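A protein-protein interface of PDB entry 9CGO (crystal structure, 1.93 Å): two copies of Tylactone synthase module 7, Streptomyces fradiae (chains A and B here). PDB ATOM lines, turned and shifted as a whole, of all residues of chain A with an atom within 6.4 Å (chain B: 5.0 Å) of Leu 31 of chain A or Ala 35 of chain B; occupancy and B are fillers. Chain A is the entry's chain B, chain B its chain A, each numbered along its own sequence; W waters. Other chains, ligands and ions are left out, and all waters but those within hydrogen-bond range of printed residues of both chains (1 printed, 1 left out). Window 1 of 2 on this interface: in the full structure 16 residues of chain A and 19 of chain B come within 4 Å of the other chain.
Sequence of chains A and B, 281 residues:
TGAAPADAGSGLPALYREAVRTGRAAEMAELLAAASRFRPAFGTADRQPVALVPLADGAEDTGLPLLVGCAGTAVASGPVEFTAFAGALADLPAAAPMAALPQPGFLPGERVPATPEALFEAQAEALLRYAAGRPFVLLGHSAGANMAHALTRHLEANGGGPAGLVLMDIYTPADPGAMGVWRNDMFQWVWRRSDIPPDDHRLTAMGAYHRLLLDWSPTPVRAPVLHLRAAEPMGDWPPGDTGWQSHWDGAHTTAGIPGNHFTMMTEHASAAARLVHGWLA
Of the printed residues of chain B, Leu 15 of chain A touches Ala 35 (3.8 Å), Phe 38 (3.8 Å) and Thr 204 (3.9 Å). Of chain B, only Leu 31 (3.8 Å), Ala 34 (3.7 Å), Ala 35 (3.5 Å) and Phe 38 (3.6 Å) come within 4 Å of Leu 31 of chain A. Of the printed residues of chain A, Ala 34 of chain B touches Leu 31 (3.7 Å). Of chain A, only Leu 15 (3.8 Å) and Leu 31 (3.5 Å) come within 4 Å of Ala 35 of chain B. The nearest residue of chain A that does not touch Ala 35 of chain B is Leu 12 of chain A (5.6 Å).
Water W1 lies within hydrogen-bond range of O of Ala 34 of chain B (2.8 Å) and OE2 of Glu 27 of chain A (2.9 Å).
The guanidinium group of Arg 39 of chain B sits at hydrogen-bond distance from the side-chain hydroxyl of Thr 204 of chain B.
Leu 31 of chain B touches its own counterpart, Leu 31 of chain A. Leu 31 of chain A touches Ala 34 of chain B, and with the chains exchanged Ala 34 of chain A touches Leu 31 of chain B. Leu 31 of chain A touches Ala 35 of chain B, and with the chains exchanged Ala 35 of chain A touches Leu 31 of chain B.
Of the 11 printed residues of chain B, 6 touch a printed residue of chain A. Along chain B the printed residues that touch a printed residue of chain A span positions 31 to 204. Of the 13 printed residues of chain A, 6 touch a printed residue of chain B. Among the printed residues, no Asp or Glu carboxylate lies within 4 Å of a Lys or Arg side-chain nitrogen of the other chain.
Among the printed residues, merely in contact across the chains: Glu 27 of chain A with Phe 38 of chain B (3.4 Å), Leu 31 of chain A with Ala 35 of chain B (3.5 Å), Ala 34 of chain A with Leu 31 of chain B (3.6 Å), Met 28 of chain A with Phe 38 of chain B (3.6 Å), Leu 31 of chain A with Phe 38 of chain B (3.6 Å), Ala 35 of chain A with Leu 31 of chain B (3.7 Å), Leu 31 of chain A with Ala 34 of chain B (3.7 Å), Leu 15 of chain A with Phe 38 of chain B (3.8 Å), Glu 27 of chain A with Arg 37 of chain B (3.8 Å), Leu 31 of chain A with Leu 31 of chain B (3.8 Å), Leu 15 of chain A with Ala 35 of chain B (3.8 Å) and Leu 15 of chain A with Thr 204 of chain B (3.9 Å).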
ATOM      1  N   LEU A  12      -1.691  10.417  -7.403  1.00  0.00           N
ATOM      2  CA  LEU A  12      -1.791  10.358  -8.860  1.00  0.00           C
ATOM      3  C   LEU A  12      -0.742   9.449  -9.498  1.00  0.00           C
ATOM      4  O   LEU A  12      -1.114   8.684 -10.404  1.00  0.00           O
ATOM      5  CB  LEU A  12      -1.724  11.775  -9.448  1.00  0.00           C
ATOM      6  CG  LEU A  12      -3.032  12.556  -9.277  1.00  0.00           C
ATOM      7  CD1 LEU A  12      -2.819  14.038  -9.487  1.00  0.00           C
ATOM      8  CD2 LEU A  12      -4.147  12.009 -10.182  1.00  0.00           C
ATOM      9  N   LEU A  15      -2.065   5.951  -9.320  1.00  0.00           N
ATOM     10  CA  LEU A  15      -3.195   5.866 -10.230  1.00  0.00           C
ATOM     11  C   LEU A  15      -2.721   5.890 -11.679  1.00  0.00           C
ATOM     12  O   LEU A  15      -3.255   5.172 -12.533  1.00  0.00           O
ATOM     13  CB  LEU A  15      -4.163   7.015  -9.941  1.00  0.00           C
ATOM     14  CG  LEU A  15      -4.807   6.913  -8.551  1.00  0.00           C
ATOM     15  CD1 LEU A  15      -5.671   8.124  -8.284  1.00  0.00           C
ATOM     16  CD2 LEU A  15      -5.626   5.618  -8.453  1.00  0.00           C
ATOM     17  N   ALA A  26      -5.739   6.857 -22.188  1.00  0.00           N
ATOM     18  CA  ALA A  26      -6.729   7.855 -22.572  1.00  0.00           C
ATOM     19  C   ALA A  26      -7.610   8.259 -21.394  1.00  0.00           C
ATOM     20  O   ALA A  26      -7.824   9.450 -21.155  1.00  0.00           O
ATOM     21  CB  ALA A  26      -7.589   7.315 -23.711  1.00  0.00           C
ATOM     22  N   GLU A  27      -8.168   7.279 -20.671  1.00  0.00           N
ATOM     23  CA  GLU A  27      -8.995   7.623 -19.515  1.00  0.00           C
ATOM     24  C   GLU A  27      -8.200   8.471 -18.531  1.00  0.00           C
ATOM     25  O   GLU A  27      -8.678   9.511 -18.074  1.00  0.00           O
ATOM     26  CB  GLU A  27      -9.542   6.361 -18.837  1.00  0.00           C
ATOM     27  CG  GLU A  27     -10.606   6.647 -17.759  1.00  0.00           C
ATOM     28  CD  GLU A  27     -11.141   5.395 -17.051  1.00  0.00           C
ATOM     29  OE1 GLU A  27     -10.709   4.266 -17.364  1.00  0.00           O
ATOM     30  OE2 GLU A  27     -12.014   5.551 -16.174  1.00  0.00           O
ATOM     31  N   MET A  28      -6.951   8.089 -18.276  1.00  0.00           N
ATOM     32  CA  MET A  28      -6.055   8.784 -17.339  1.00  0.00           C
ATOM     33  C   MET A  28      -5.665  10.186 -17.781  1.00  0.00           C
ATOM     34  O   MET A  28      -5.608  11.098 -16.965  1.00  0.00           O
ATOM     35  CB  MET A  28      -4.796   7.946 -17.119  1.00  0.00           C
ATOM     36  CG  MET A  28      -3.659   8.619 -16.343  1.00  0.00           C
ATOM     37  SD  MET A  28      -4.055   9.131 -14.459  1.00  0.00           S
ATOM     38  CE  MET A  28      -4.992   7.527 -13.889  1.00  0.00           C
ATOM     39  N   ALA A  29      -5.389  10.358 -19.077  1.00  0.00           N
ATOM     40  CA  ALA A  29      -5.061  11.685 -19.587  1.00  0.00           C
ATOM     41  C   ALA A  29      -6.196  12.659 -19.314  1.00  0.00           C
ATOM     42  O   ALA A  29      -5.963  13.791 -18.871  1.00  0.00           O
ATOM     43  CB  ALA A  29      -4.767  11.611 -21.090  1.00  0.00           C
ATOM     44  N   GLU A  30      -7.429  12.236 -19.599  1.00  0.00           N
ATOM     45  CA  GLU A  30      -8.612  13.016 -19.248  1.00  0.00           C
ATOM     46  C   GLU A  30      -8.661  13.316 -17.749  1.00  0.00           C
ATOM     47  O   GLU A  30      -8.920  14.452 -17.337  1.00  0.00           O
ATOM     48  CB  GLU A  30      -9.866  12.256 -19.687  1.00  0.00           C
ATOM     49  CG  GLU A  30     -10.905  13.129 -20.357  1.00  0.00           C
ATOM     50  CD  GLU A  30     -11.999  12.333 -21.053  1.00  0.00           C
ATOM     51  OE1 GLU A  30     -11.788  11.136 -21.350  1.00  0.00           O
ATOM     52  OE2 GLU A  30     -13.072  12.916 -21.308  1.00  0.00           O
ATOM     53  N   LEU A  31      -8.430  12.299 -16.918  1.00  0.00           N
ATOM     54  CA  LEU A  31      -8.338  12.525 -15.478  1.00  0.00           C
ATOM     55  C   LEU A  31      -7.335  13.627 -15.170  1.00  0.00           C
ATOM     56  O   LEU A  31      -7.635  14.577 -14.439  1.00  0.00           O
ATOM     57  CB  LEU A  31      -7.948  11.225 -14.776  1.00  0.00           C
ATOM     58  CG  LEU A  31      -7.999  11.173 -13.244  1.00  0.00           C
ATOM     59  CD1 LEU A  31      -9.382  11.546 -12.736  1.00  0.00           C
ATOM     60  CD2 LEU A  31      -7.638   9.783 -12.802  1.00  0.00           C
ATOM     61  N   LEU A  32      -6.144  13.539 -15.764  1.00  0.00           N
ATOM     62  CA  LEU A  32      -5.121  14.526 -15.467  1.00  0.00           C
ATOM     63  C   LEU A  32      -5.519  15.890 -15.996  1.00  0.00           C
ATOM     64  O   LEU A  32      -5.246  16.906 -15.351  1.00  0.00           O
ATOM     65  CB  LEU A  32      -3.769  14.079 -16.032  1.00  0.00           C
ATOM     66  CG  LEU A  32      -3.128  12.819 -15.426  1.00  0.00           C
ATOM     67  CD1 LEU A  32      -1.952  12.359 -16.267  1.00  0.00           C
ATOM     68  CD2 LEU A  32      -2.669  13.056 -13.970  1.00  0.00           C
ATOM     69  N   ALA A  33      -6.170  15.943 -17.167  1.00  0.00           N
ATOM     70  CA  ALA A  33      -6.605  17.241 -17.680  1.00  0.00           C
ATOM     71  C   ALA A  33      -7.695  17.848 -16.799  1.00  0.00           C
ATOM     72  O   ALA A  33      -7.712  19.061 -16.571  1.00  0.00           O
ATOM     73  CB  ALA A  33      -7.073  17.118 -19.135  1.00  0.00           C
ATOM     74  N   ALA A  34      -8.607  17.025 -16.271  1.00  0.00           N
ATOM     75  CA  ALA A  34      -9.606  17.558 -15.350  1.00  0.00           C
ATOM     76  C   ALA A  34      -8.975  17.991 -14.032  1.00  0.00           C
ATOM     77  O   ALA A  34      -9.411  18.978 -13.434  1.00  0.00           O
ATOM     78  CB  ALA A  34     -10.706  16.521 -15.097  1.00  0.00           C
ATOM     79  N   ALA A  35      -7.947  17.275 -13.576  1.00  0.00           N
ATOM     80  CA  ALA A  35      -7.258  17.635 -12.332  1.00  0.00           C
ATOM     81  C   ALA A  35      -6.580  18.992 -12.417  1.00  0.00           C
ATOM     82  O   ALA A  35      -6.519  19.737 -11.425  1.00  0.00           O
ATOM     83  CB  ALA A  35      -6.215  16.575 -11.999  1.00  0.00           C
ATOM     84  N   SER A  36      -6.005  19.311 -13.577  1.00  0.00           N
ATOM     85  CA  SER A  36      -5.261  20.555 -13.713  1.00  0.00           C
ATOM     86  C   SER A  36      -6.148  21.772 -13.566  1.00  0.00           C
ATOM     87  O   SER A  36      -5.642  22.889 -13.425  1.00  0.00           O
ATOM     88  CB  SER A  36      -4.580  20.588 -15.076  1.00  0.00           C
ATOM     89  OG  SER A  36      -5.579  20.529 -16.086  1.00  0.00           O
ATOM     90  N   LEU B  12      -3.580  15.014  -4.716  1.00  0.00           N
ATOM     91  CA  LEU B  12      -5.025  15.157  -4.524  1.00  0.00           C
ATOM     92  C   LEU B  12      -5.433  15.813  -3.201  1.00  0.00           C
ATOM     93  O   LEU B  12      -6.500  16.452  -3.178  1.00  0.00           O
ATOM     94  CB  LEU B  12      -5.704  13.779  -4.639  1.00  0.00           C
ATOM     95  CG  LEU B  12      -5.518  12.964  -5.929  1.00  0.00           C
ATOM     96  CD1 LEU B  12      -5.964  11.522  -5.738  1.00  0.00           C
ATOM     97  CD2 LEU B  12      -6.245  13.609  -7.102  1.00  0.00           C
ATOM     98  N   LEU B  31     -14.223  14.694  -9.798  1.00  0.00           N
ATOM     99  CA  LEU B  31     -12.860  14.248 -10.093  1.00  0.00           C
ATOM    100  C   LEU B  31     -12.518  12.987  -9.314  1.00  0.00           C
ATOM    101  O   LEU B  31     -11.961  12.031  -9.867  1.00  0.00           O
ATOM    102  CB  LEU B  31     -11.844  15.337  -9.769  1.00  0.00           C
ATOM    103  CG  LEU B  31     -10.433  14.973 -10.248  1.00  0.00           C
ATOM    104  CD1 LEU B  31     -10.326  15.163 -11.768  1.00  0.00           C
ATOM    105  CD2 LEU B  31      -9.348  15.773  -9.504  1.00  0.00           C
ATOM    106  N   LEU B  32     -12.825  12.975  -8.019  1.00  0.00           N
ATOM    107  CA  LEU B  32     -12.481  11.826  -7.194  1.00  0.00           C
ATOM    108  C   LEU B  32     -13.253  10.592  -7.614  1.00  0.00           C
ATOM    109  O   LEU B  32     -12.729   9.476  -7.519  1.00  0.00           O
ATOM    110  CB  LEU B  32     -12.740  12.131  -5.720  1.00  0.00           C
ATOM    111  CG  LEU B  32     -11.907  13.216  -5.041  1.00  0.00           C
ATOM    112  CD1 LEU B  32     -12.305  13.289  -3.600  1.00  0.00           C
ATOM    113  CD2 LEU B  32     -10.403  12.937  -5.169  1.00  0.00           C
ATOM    114  N   ALA B  33     -14.503  10.765  -8.055  1.00  0.00           N
ATOM    115  CA  ALA B  33     -15.240   9.650  -8.635  1.00  0.00           C
ATOM    116  C   ALA B  33     -14.468   9.056  -9.806  1.00  0.00           C
ATOM    117  O   ALA B  33     -14.262   7.841  -9.882  1.00  0.00           O
ATOM    118  CB  ALA B  33     -16.636  10.111  -9.071  1.00  0.00           C
ATOM    119  N   ALA B  34     -14.005   9.919 -10.714  1.00  0.00           N
ATOM    120  CA  ALA B  34     -13.225   9.480 -11.866  1.00  0.00           C
ATOM    121  C   ALA B  34     -11.895   8.881 -11.443  1.00  0.00           C
ATOM    122  O   ALA B  34     -11.494   7.819 -11.943  1.00  0.00           O
ATOM    123  CB  ALA B  34     -12.982  10.661 -12.813  1.00  0.00           C
ATOM    124  N   ALA B  35     -11.189   9.561 -10.535  1.00  0.00           N
ATOM    125  CA  ALA B  35      -9.880   9.091 -10.086  1.00  0.00           C
ATOM    126  C   ALA B  35      -9.983   7.717  -9.450  1.00  0.00           C
ATOM    127  O   ALA B  35      -9.079   6.879  -9.595  1.00  0.00           O
ATOM    128  CB  ALA B  35      -9.285  10.088  -9.097  1.00  0.00           C
ATOM    129  N   SER B  36     -11.089   7.466  -8.740  1.00  0.00           N
ATOM    130  CA  SER B  36     -11.307   6.202  -8.051  1.00  0.00           C
ATOM    131  C   SER B  36     -11.516   5.038  -9.005  1.00  0.00           C
ATOM    132  O   SER B  36     -11.278   3.891  -8.619  1.00  0.00           O
ATOM    133  CB  SER B  36     -12.525   6.321  -7.131  1.00  0.00           C
ATOM    134  OG  SER B  36     -13.735   6.315  -7.887  1.00  0.00           O
ATOM    135  N   ARG B  37     -11.963   5.289 -10.242  1.00  0.00           N
ATOM    136  CA  ARG B  37     -12.128   4.174 -11.173  1.00  0.00           C
ATOM    137  C   ARG B  37     -10.810   3.505 -11.509  1.00  0.00           C
ATOM    138  O   ARG B  37     -10.808   2.520 -12.243  1.00  0.00           O
ATOM    139  CB  ARG B  37     -12.805   4.627 -12.471  1.00  0.00           C
ATOM    140  CG  ARG B  37     -14.296   4.849 -12.354  1.00  0.00           C
ATOM    141  CD  ARG B  37     -14.899   5.171 -13.701  1.00  0.00           C
ATOM    142  NE  ARG B  37     -16.301   5.559 -13.589  1.00  0.00           N
ATOM    143  CZ  ARG B  37     -16.767   6.784 -13.804  1.00  0.00           C
ATOM    144  NH1 ARG B  37     -15.969   7.770 -14.186  1.00  0.00           N
ATOM    145  NH2 ARG B  37     -18.067   7.025 -13.642  1.00  0.00           N
ATOM    146  N   PHE B  38      -9.697   4.013 -11.004  1.00  0.00           N
ATOM    147  CA  PHE B  38      -8.419   3.338 -11.133  1.00  0.00           C
ATOM    148  C   PHE B  38      -7.985   2.629  -9.846  1.00  0.00           C
ATOM    149  O   PHE B  38      -6.911   2.016  -9.830  1.00  0.00           O
ATOM    150  CB  PHE B  38      -7.354   4.349 -11.591  1.00  0.00           C
ATOM    151  CG  PHE B  38      -7.673   5.008 -12.923  1.00  0.00           C
ATOM    152  CD1 PHE B  38      -8.577   6.060 -12.998  1.00  0.00           C
ATOM    153  CD2 PHE B  38      -7.080   4.565 -14.093  1.00  0.00           C
ATOM    154  CE1 PHE B  38      -8.873   6.655 -14.199  1.00  0.00           C
ATOM    155  CE2 PHE B  38      -7.372   5.162 -15.303  1.00  0.00           C
ATOM    156  CZ  PHE B  38      -8.266   6.207 -15.355  1.00  0.00           C
ATOM    157  N   ARG B  39      -8.795   2.686  -8.778  1.00  0.00           N
ATOM    158  CA  ARG B  39      -8.479   1.962  -7.541  1.00  0.00           C
ATOM    159  C   ARG B  39      -8.660   0.461  -7.732  1.00  0.00           C
ATOM    160  O   ARG B  39      -9.636   0.025  -8.347  1.00  0.00           O
ATOM    161  CB  ARG B  39      -9.370   2.417  -6.382  1.00  0.00           C
ATOM    162  CG  ARG B  39      -9.072   3.784  -5.824  1.00  0.00           C
ATOM    163  CD  ARG B  39      -7.938   3.740  -4.833  1.00  0.00           C
ATOM    164  NE  ARG B  39      -8.160   2.785  -3.750  1.00  0.00           N
ATOM    165  CZ  ARG B  39      -8.517   3.109  -2.515  1.00  0.00           C
ATOM    166  NH1 ARG B  39      -8.709   4.369  -2.155  1.00  0.00           N
ATOM    167  NH2 ARG B  39      -8.675   2.144  -1.618  1.00  0.00           N
ATOM    168  N   THR B 204      -9.549   9.098  -2.531  1.00  0.00           N
ATOM    169  CA  THR B 204      -9.939   8.192  -3.603  1.00  0.00           C
ATOM    170  C   THR B 204     -10.993   7.191  -3.134  1.00  0.00           C
ATOM    171  O   THR B 204     -11.844   6.782  -3.928  1.00  0.00           O
ATOM    172  CB  THR B 204      -8.702   7.495  -4.211  1.00  0.00           C
ATOM    173  OG1 THR B 204      -7.817   7.006  -3.193  1.00  0.00           O
ATOM    174  CG2 THR B 204      -7.910   8.502  -5.070  1.00  0.00           C
HETATM  175  O   HOH W   1     -11.939   7.982 -14.676  1.00  0.00           O
